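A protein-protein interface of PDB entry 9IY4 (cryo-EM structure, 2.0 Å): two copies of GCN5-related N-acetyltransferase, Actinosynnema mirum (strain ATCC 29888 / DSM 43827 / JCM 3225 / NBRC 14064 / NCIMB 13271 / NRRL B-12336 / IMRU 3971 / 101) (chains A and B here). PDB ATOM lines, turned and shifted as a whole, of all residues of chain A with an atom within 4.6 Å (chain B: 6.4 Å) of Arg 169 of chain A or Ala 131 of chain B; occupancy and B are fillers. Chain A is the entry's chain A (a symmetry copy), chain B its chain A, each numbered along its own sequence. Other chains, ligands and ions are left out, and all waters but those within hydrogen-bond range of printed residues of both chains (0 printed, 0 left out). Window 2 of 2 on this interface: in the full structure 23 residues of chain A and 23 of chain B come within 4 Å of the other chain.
The guanidinium group (NE) of Arg 95 of chain B is in hydrogen-bond range of the backbone carbonyl oxygen (O) of Ala 129 of chain B (3.3 Å).
The backbone carbonyl oxygen (O) of Arg 95 of chain B sits at hydrogen-bond distance from the backbone NH (N) of Ala 131 of chain B, at 2.7 Å.
N of Ser 162 of chain A lies within hydrogen-bond range of O of Val 170 of chain A, at 3.2 Å.
No position is printed for both chains.
Of the 9 pairs that touch across the chains among the printed residues, none has its exchanged pair printed and touching as well.
Of the 8 printed residues of chain A, 4 touch a printed residue of chain B.
Printed residues of chain A that touch a printed residue of chain B: Asp 161, Ser 162, Phe 164 and Arg 169.
Of the 15 printed residues of chain B, 7 touch a printed residue of chain A.
Printed residues of chain B that touch a printed residue of chain A: His 93, Val 94, Arg 95, Thr 96, Ala 131, Cys 132 and Glu 180.
Hydrophobic or aromatic side chains of chain B that line the printed part of chain A: Ala 131.
Among the printed residues, 9 pairs touch across the chains.
Among the printed residues, no Asp or Glu carboxylate lies within 4 Å of a Lys or Arg side-chain nitrogen of the other chain.
Arg 169 of chain A touches three residues of chain B.
Of chain A, only Asp 161 (3.9 Å) and Arg 169 (3.5 Å) come within 4 Å of Ala 131 of chain B.
Of the printed residues of chain B, Ser 162 of chain A touches Thr 96 (3.7 Å).
Of the printed residues of chain A, Glu 180 of chain B touches Asp 161 (3.5 Å).
The nearest residue of chain B that does not touch Arg 169 of chain A is Thr 96 of chain B (4.5 Å).
The nearest printed residue of chain A that does not touch His 93 of chain B is Arg 169 of chain A (6.2 Å).
The backbone carbonyl oxygen (O) of Val 94 of chain B is in hydrogen-bond range of the guanidinium group (NH1) of Arg 169 of chain A.
The side-chain carboxylate (OE2) of Glu 180 of chain B sits close to the side-chain carboxylate (OD2) of Asp 161 of chain A, 3.5 Å away.
Among the printed residues, merely in contact across the chains: Asp 161 of chain A with Cys 132 of chain B (3.2 Å), Arg 169 of chain A with Arg 95 of chain B (3.4 Å), Arg 169 of chain A with Ala 131 of chain B (3.5 Å), Ser 162 of chain A with Thr 96 of chain B (3.7 Å), Phe 164 of chain A with His 93 of chain B (3.9 Å), Asp 161 of chain A with Ala 131 of chain B (3.9 Å) and Phe 164 of chain A with Val 94 of chain B (3.9 Å).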
ATOM      1  N   ASP A 161      -2.463 -17.664 -22.516  1.00  0.00           N
ATOM      2  CA  ASP A 161      -3.097 -17.822 -21.206  1.00  0.00           C
ATOM      3  C   ASP A 161      -2.116 -17.570 -20.063  1.00  0.00           C
ATOM      4  O   ASP A 161      -1.893 -18.415 -19.198  1.00  0.00           O
ATOM      5  CB  ASP A 161      -3.727 -19.209 -21.080  1.00  0.00           C
ATOM      6  CG  ASP A 161      -4.767 -19.473 -22.142  1.00  0.00           C
ATOM      7  OD1 ASP A 161      -5.191 -18.511 -22.811  1.00  0.00           O
ATOM      8  OD2 ASP A 161      -5.164 -20.644 -22.307  1.00  0.00           O
ATOM      9  N   SER A 162      -1.541 -16.370 -20.055  1.00  0.00           N
ATOM     10  CA  SER A 162      -0.513 -16.032 -19.082  1.00  0.00           C
ATOM     11  C   SER A 162      -0.788 -14.705 -18.386  1.00  0.00           C
ATOM     12  O   SER A 162       0.133 -14.101 -17.832  1.00  0.00           O
ATOM     13  CB  SER A 162       0.862 -15.999 -19.744  1.00  0.00           C
ATOM     14  OG  SER A 162       0.935 -14.950 -20.683  1.00  0.00           O
ATOM     15  N   GLY A 163      -2.030 -14.240 -18.400  1.00  0.00           N
ATOM     16  CA  GLY A 163      -2.379 -13.026 -17.690  1.00  0.00           C
ATOM     17  C   GLY A 163      -3.876 -12.842 -17.667  1.00  0.00           C
ATOM     18  O   GLY A 163      -4.624 -13.543 -18.353  1.00  0.00           O
ATOM     19  N   PHE A 164      -4.307 -11.875 -16.864  1.00  0.00           N
ATOM     20  CA  PHE A 164      -5.715 -11.533 -16.734  1.00  0.00           C
ATOM     21  C   PHE A 164      -5.940 -10.113 -17.219  1.00  0.00           C
ATOM     22  O   PHE A 164      -5.182  -9.205 -16.866  1.00  0.00           O
ATOM     23  CB  PHE A 164      -6.205 -11.654 -15.291  1.00  0.00           C
ATOM     24  CG  PHE A 164      -6.282 -13.056 -14.787  1.00  0.00           C
ATOM     25  CD1 PHE A 164      -7.394 -13.831 -15.047  1.00  0.00           C
ATOM     26  CD2 PHE A 164      -5.280 -13.577 -13.999  1.00  0.00           C
ATOM     27  CE1 PHE A 164      -7.478 -15.113 -14.576  1.00  0.00           C
ATOM     28  CE2 PHE A 164      -5.365 -14.857 -13.519  1.00  0.00           C
ATOM     29  CZ  PHE A 164      -6.465 -15.625 -13.808  1.00  0.00           C
ATOM     30  N   GLY A 167     -10.331  -9.662 -15.535  1.00  0.00           N
ATOM     31  CA  GLY A 167     -10.793 -10.939 -15.046  1.00  0.00           C
ATOM     32  C   GLY A 167     -10.802 -12.046 -16.071  1.00  0.00           C
ATOM     33  O   GLY A 167     -10.985 -13.209 -15.699  1.00  0.00           O
ATOM     34  N   ARG A 168     -10.607 -11.722 -17.341  1.00  0.00           N
ATOM     35  CA  ARG A 168     -10.599 -12.704 -18.412  1.00  0.00           C
ATOM     36  C   ARG A 168      -9.175 -13.188 -18.640  1.00  0.00           C
ATOM     37  O   ARG A 168      -8.233 -12.393 -18.611  1.00  0.00           O
ATOM     38  CB  ARG A 168     -11.173 -12.089 -19.688  1.00  0.00           C
ATOM     39  CG  ARG A 168     -11.214 -13.012 -20.883  1.00  0.00           C
ATOM     40  CD  ARG A 168     -12.068 -12.410 -21.986  1.00  0.00           C
ATOM     41  NE  ARG A 168     -11.548 -11.122 -22.428  1.00  0.00           N
ATOM     42  CZ  ARG A 168     -10.682 -10.959 -23.418  1.00  0.00           C
ATOM     43  NH1 ARG A 168     -10.234 -11.986 -24.120  1.00  0.00           N
ATOM     44  NH2 ARG A 168     -10.258  -9.734 -23.714  1.00  0.00           N
ATOM     45  N   ARG A 169      -9.019 -14.493 -18.838  1.00  0.00           N
ATOM     46  CA  ARG A 169      -7.712 -15.060 -19.139  1.00  0.00           C
ATOM     47  C   ARG A 169      -7.326 -14.748 -20.581  1.00  0.00           C
ATOM     48  O   ARG A 169      -8.021 -15.149 -21.519  1.00  0.00           O
ATOM     49  CB  ARG A 169      -7.729 -16.564 -18.880  1.00  0.00           C
ATOM     50  CG  ARG A 169      -6.449 -17.283 -19.231  1.00  0.00           C
ATOM     51  CD  ARG A 169      -5.381 -17.048 -18.194  1.00  0.00           C
ATOM     52  NE  ARG A 169      -5.599 -17.789 -16.962  1.00  0.00           N
ATOM     53  CZ  ARG A 169      -4.742 -17.804 -15.952  1.00  0.00           C
ATOM     54  NH1 ARG A 169      -3.586 -17.168 -16.020  1.00  0.00           N
ATOM     55  NH2 ARG A 169      -5.055 -18.470 -14.847  1.00  0.00           N
ATOM     56  N   VAL A 170      -6.217 -14.027 -20.755  1.00  0.00           N
ATOM     57  CA  VAL A 170      -5.748 -13.576 -22.058  1.00  0.00           C
ATOM     58  C   VAL A 170      -4.259 -13.877 -22.178  1.00  0.00           C
ATOM     59  O   VAL A 170      -3.578 -14.164 -21.196  1.00  0.00           O
ATOM     60  CB  VAL A 170      -6.002 -12.073 -22.289  1.00  0.00           C
ATOM     61  CG1 VAL A 170      -7.482 -11.770 -22.255  1.00  0.00           C
ATOM     62  CG2 VAL A 170      -5.274 -11.253 -21.243  1.00  0.00           C
ATOM     63  N   HIS B  93      -0.015 -15.401  -8.827  1.00  0.00           N
ATOM     64  CA  HIS B  93      -0.948 -14.336  -9.174  1.00  0.00           C
ATOM     65  C   HIS B  93      -1.647 -14.599 -10.500  1.00  0.00           C
ATOM     66  O   HIS B  93      -2.794 -14.181 -10.683  1.00  0.00           O
ATOM     67  CB  HIS B  93      -0.214 -13.001  -9.217  1.00  0.00           C
ATOM     68  CG  HIS B  93       0.172 -12.487  -7.868  1.00  0.00           C
ATOM     69  ND1 HIS B  93      -0.497 -11.457  -7.247  1.00  0.00           N
ATOM     70  CD2 HIS B  93       1.148 -12.870  -7.015  1.00  0.00           C
ATOM     71  CE1 HIS B  93       0.055 -11.223  -6.070  1.00  0.00           C
ATOM     72  NE2 HIS B  93       1.055 -12.067  -5.905  1.00  0.00           N
ATOM     73  N   VAL B  94      -0.984 -15.281 -11.437  1.00  0.00           N
ATOM     74  CA  VAL B  94      -1.548 -15.525 -12.757  1.00  0.00           C
ATOM     75  C   VAL B  94      -1.605 -17.002 -13.116  1.00  0.00           C
ATOM     76  O   VAL B  94      -1.985 -17.332 -14.238  1.00  0.00           O
ATOM     77  CB  VAL B  94      -0.786 -14.743 -13.845  1.00  0.00           C
ATOM     78  CG1 VAL B  94      -0.988 -13.257 -13.658  1.00  0.00           C
ATOM     79  CG2 VAL B  94       0.684 -15.069 -13.801  1.00  0.00           C
ATOM     80  N   ARG B  95      -1.250 -17.903 -12.197  1.00  0.00           N
ATOM     81  CA  ARG B  95      -1.318 -19.348 -12.430  1.00  0.00           C
ATOM     82  C   ARG B  95      -0.384 -19.788 -13.556  1.00  0.00           C
ATOM     83  O   ARG B  95      -0.758 -20.594 -14.406  1.00  0.00           O
ATOM     84  CB  ARG B  95      -2.754 -19.805 -12.723  1.00  0.00           C
ATOM     85  CG  ARG B  95      -3.835 -19.300 -11.771  1.00  0.00           C
ATOM     86  CD  ARG B  95      -3.422 -19.483 -10.336  1.00  0.00           C
ATOM     87  NE  ARG B  95      -3.175 -20.890 -10.061  1.00  0.00           N
ATOM     88  CZ  ARG B  95      -2.565 -21.346  -8.980  1.00  0.00           C
ATOM     89  NH1 ARG B  95      -2.087 -20.526  -8.063  1.00  0.00           N
ATOM     90  NH2 ARG B  95      -2.406 -22.655  -8.831  1.00  0.00           N
ATOM     91  N   THR B  96       0.840 -19.265 -13.570  1.00  0.00           N
ATOM     92  CA  THR B  96       1.828 -19.654 -14.568  1.00  0.00           C
ATOM     93  C   THR B  96       3.124 -20.070 -13.892  1.00  0.00           C
ATOM     94  O   THR B  96       3.396 -19.710 -12.747  1.00  0.00           O
ATOM     95  CB  THR B  96       2.129 -18.533 -15.577  1.00  0.00           C
ATOM     96  OG1 THR B  96       2.758 -17.436 -14.908  1.00  0.00           O
ATOM     97  CG2 THR B  96       0.865 -18.061 -16.267  1.00  0.00           C
ATOM     98  N   ALA B 124       2.013 -30.016 -12.871  1.00  0.00           N
ATOM     99  CA  ALA B 124       1.760 -28.580 -12.820  1.00  0.00           C
ATOM    100  C   ALA B 124       0.334 -28.247 -13.235  1.00  0.00           C
ATOM    101  O   ALA B 124      -0.267 -27.309 -12.705  1.00  0.00           O
ATOM    102  CB  ALA B 124       2.763 -27.841 -13.699  1.00  0.00           C
ATOM    103  N   PHE B 125      -0.217 -28.991 -14.195  1.00  0.00           N
ATOM    104  CA  PHE B 125      -1.569 -28.722 -14.664  1.00  0.00           C
ATOM    105  C   PHE B 125      -2.627 -29.278 -13.716  1.00  0.00           C
ATOM    106  O   PHE B 125      -3.630 -28.611 -13.447  1.00  0.00           O
ATOM    107  CB  PHE B 125      -1.777 -29.316 -16.057  1.00  0.00           C
ATOM    108  CG  PHE B 125      -1.033 -28.605 -17.146  1.00  0.00           C
ATOM    109  CD1 PHE B 125      -0.708 -27.270 -17.029  1.00  0.00           C
ATOM    110  CD2 PHE B 125      -0.696 -29.269 -18.311  1.00  0.00           C
ATOM    111  CE1 PHE B 125      -0.034 -26.621 -18.038  1.00  0.00           C
ATOM    112  CE2 PHE B 125      -0.027 -28.623 -19.321  1.00  0.00           C
ATOM    113  CZ  PHE B 125       0.304 -27.299 -19.183  1.00  0.00           C
ATOM    114  N   ALA B 129      -2.682 -26.686 -10.667  1.00  0.00           N
ATOM    115  CA  ALA B 129      -3.712 -25.939 -11.389  1.00  0.00           C
ATOM    116  C   ALA B 129      -3.140 -24.701 -12.076  1.00  0.00           C
ATOM    117  O   ALA B 129      -3.668 -23.595 -11.959  1.00  0.00           O
ATOM    118  CB  ALA B 129      -4.863 -25.563 -10.458  1.00  0.00           C
ATOM    119  N   LEU B 130      -2.049 -24.897 -12.812  1.00  0.00           N
ATOM    120  CA  LEU B 130      -1.449 -23.828 -13.597  1.00  0.00           C
ATOM    121  C   LEU B 130      -2.095 -23.750 -14.970  1.00  0.00           C
ATOM    122  O   LEU B 130      -2.418 -24.773 -15.577  1.00  0.00           O
ATOM    123  CB  LEU B 130       0.054 -24.038 -13.752  1.00  0.00           C
ATOM    124  CG  LEU B 130       0.895 -24.110 -12.489  1.00  0.00           C
ATOM    125  CD1 LEU B 130       2.348 -24.126 -12.864  1.00  0.00           C
ATOM    126  CD2 LEU B 130       0.594 -22.926 -11.615  1.00  0.00           C
ATOM    127  N   ALA B 131      -2.282 -22.527 -15.454  1.00  0.00           N
ATOM    128  CA  ALA B 131      -2.876 -22.310 -16.763  1.00  0.00           C
ATOM    129  C   ALA B 131      -1.858 -22.308 -17.891  1.00  0.00           C
ATOM    130  O   ALA B 131      -2.235 -22.524 -19.045  1.00  0.00           O
ATOM    131  CB  ALA B 131      -3.648 -20.990 -16.778  1.00  0.00           C
ATOM    132  N   CYS B 132      -0.585 -22.069 -17.590  1.00  0.00           N
ATOM    133  CA  CYS B 132       0.438 -21.965 -18.617  1.00  0.00           C
ATOM    134  C   CYS B 132       1.795 -22.254 -18.000  1.00  0.00           C
ATOM    135  O   CYS B 132       2.126 -21.719 -16.943  1.00  0.00           O
ATOM    136  CB  CYS B 132       0.440 -20.573 -19.255  1.00  0.00           C
ATOM    137  SG  CYS B 132       1.628 -20.346 -20.589  1.00  0.00           S
ATOM    138  N   VAL B 133       2.573 -23.098 -18.667  1.00  0.00           N
ATOM    139  CA  VAL B 133       3.965 -23.336 -18.319  1.00  0.00           C
ATOM    140  C   VAL B 133       4.810 -22.925 -19.515  1.00  0.00           C
ATOM    141  O   VAL B 133       4.531 -23.340 -20.644  1.00  0.00           O
ATOM    142  CB  VAL B 133       4.218 -24.806 -17.944  1.00  0.00           C
ATOM    143  CG1 VAL B 133       5.679 -25.024 -17.639  1.00  0.00           C
ATOM    144  CG2 VAL B 133       3.366 -25.207 -16.760  1.00  0.00           C
ATOM    145  N   ALA B 177       3.166 -24.121 -22.902  1.00  0.00           N
ATOM    146  CA  ALA B 177       2.283 -25.274 -22.922  1.00  0.00           C
ATOM    147  C   ALA B 177       1.020 -24.944 -22.147  1.00  0.00           C
ATOM    148  O   ALA B 177       1.081 -24.272 -21.116  1.00  0.00           O
ATOM    149  CB  ALA B 177       2.964 -26.503 -22.318  1.00  0.00           C
ATOM    150  N   VAL B 178      -0.118 -25.424 -22.637  1.00  0.00           N
ATOM    151  CA  VAL B 178      -1.401 -25.167 -21.987  1.00  0.00           C
ATOM    152  C   VAL B 178      -2.102 -26.492 -21.722  1.00  0.00           C
ATOM    153  O   VAL B 178      -1.851 -27.475 -22.430  1.00  0.00           O
ATOM    154  CB  VAL B 178      -2.280 -24.231 -22.830  1.00  0.00           C
ATOM    155  CG1 VAL B 178      -1.643 -22.863 -22.934  1.00  0.00           C
ATOM    156  CG2 VAL B 178      -2.520 -24.822 -24.204  1.00  0.00           C
ATOM    157  N   PRO B 179      -2.976 -26.566 -20.715  1.00  0.00           N
ATOM    158  CA  PRO B 179      -3.624 -27.844 -20.389  1.00  0.00           C
ATOM    159  C   PRO B 179      -4.367 -28.485 -21.545  1.00  0.00           C
ATOM    160  O   PRO B 179      -4.358 -29.714 -21.666  1.00  0.00           O
ATOM    161  CB  PRO B 179      -4.581 -27.450 -19.262  1.00  0.00           C
ATOM    162  CG  PRO B 179      -3.902 -26.333 -18.600  1.00  0.00           C
ATOM    163  CD  PRO B 179      -3.276 -25.539 -19.704  1.00  0.00           C
ATOM    164  N   GLU B 180      -5.021 -27.695 -22.396  1.00  0.00           N
ATOM    165  CA  GLU B 180      -5.778 -28.284 -23.492  1.00  0.00           C
ATOM    166  C   GLU B 180      -4.885 -28.889 -24.568  1.00  0.00           C
ATOM    167  O   GLU B 180      -5.397 -29.578 -25.454  1.00  0.00           O
ATOM    168  CB  GLU B 180      -6.720 -27.247 -24.110  1.00  0.00           C
ATOM    169  CG  GLU B 180      -6.065 -25.958 -24.580  1.00  0.00           C
ATOM    170  CD  GLU B 180      -6.048 -24.876 -23.512  1.00  0.00           C
ATOM    171  OE1 GLU B 180      -6.296 -25.191 -22.328  1.00  0.00           O
ATOM    172  OE2 GLU B 180      -5.807 -23.701 -23.862  1.00  0.00           O
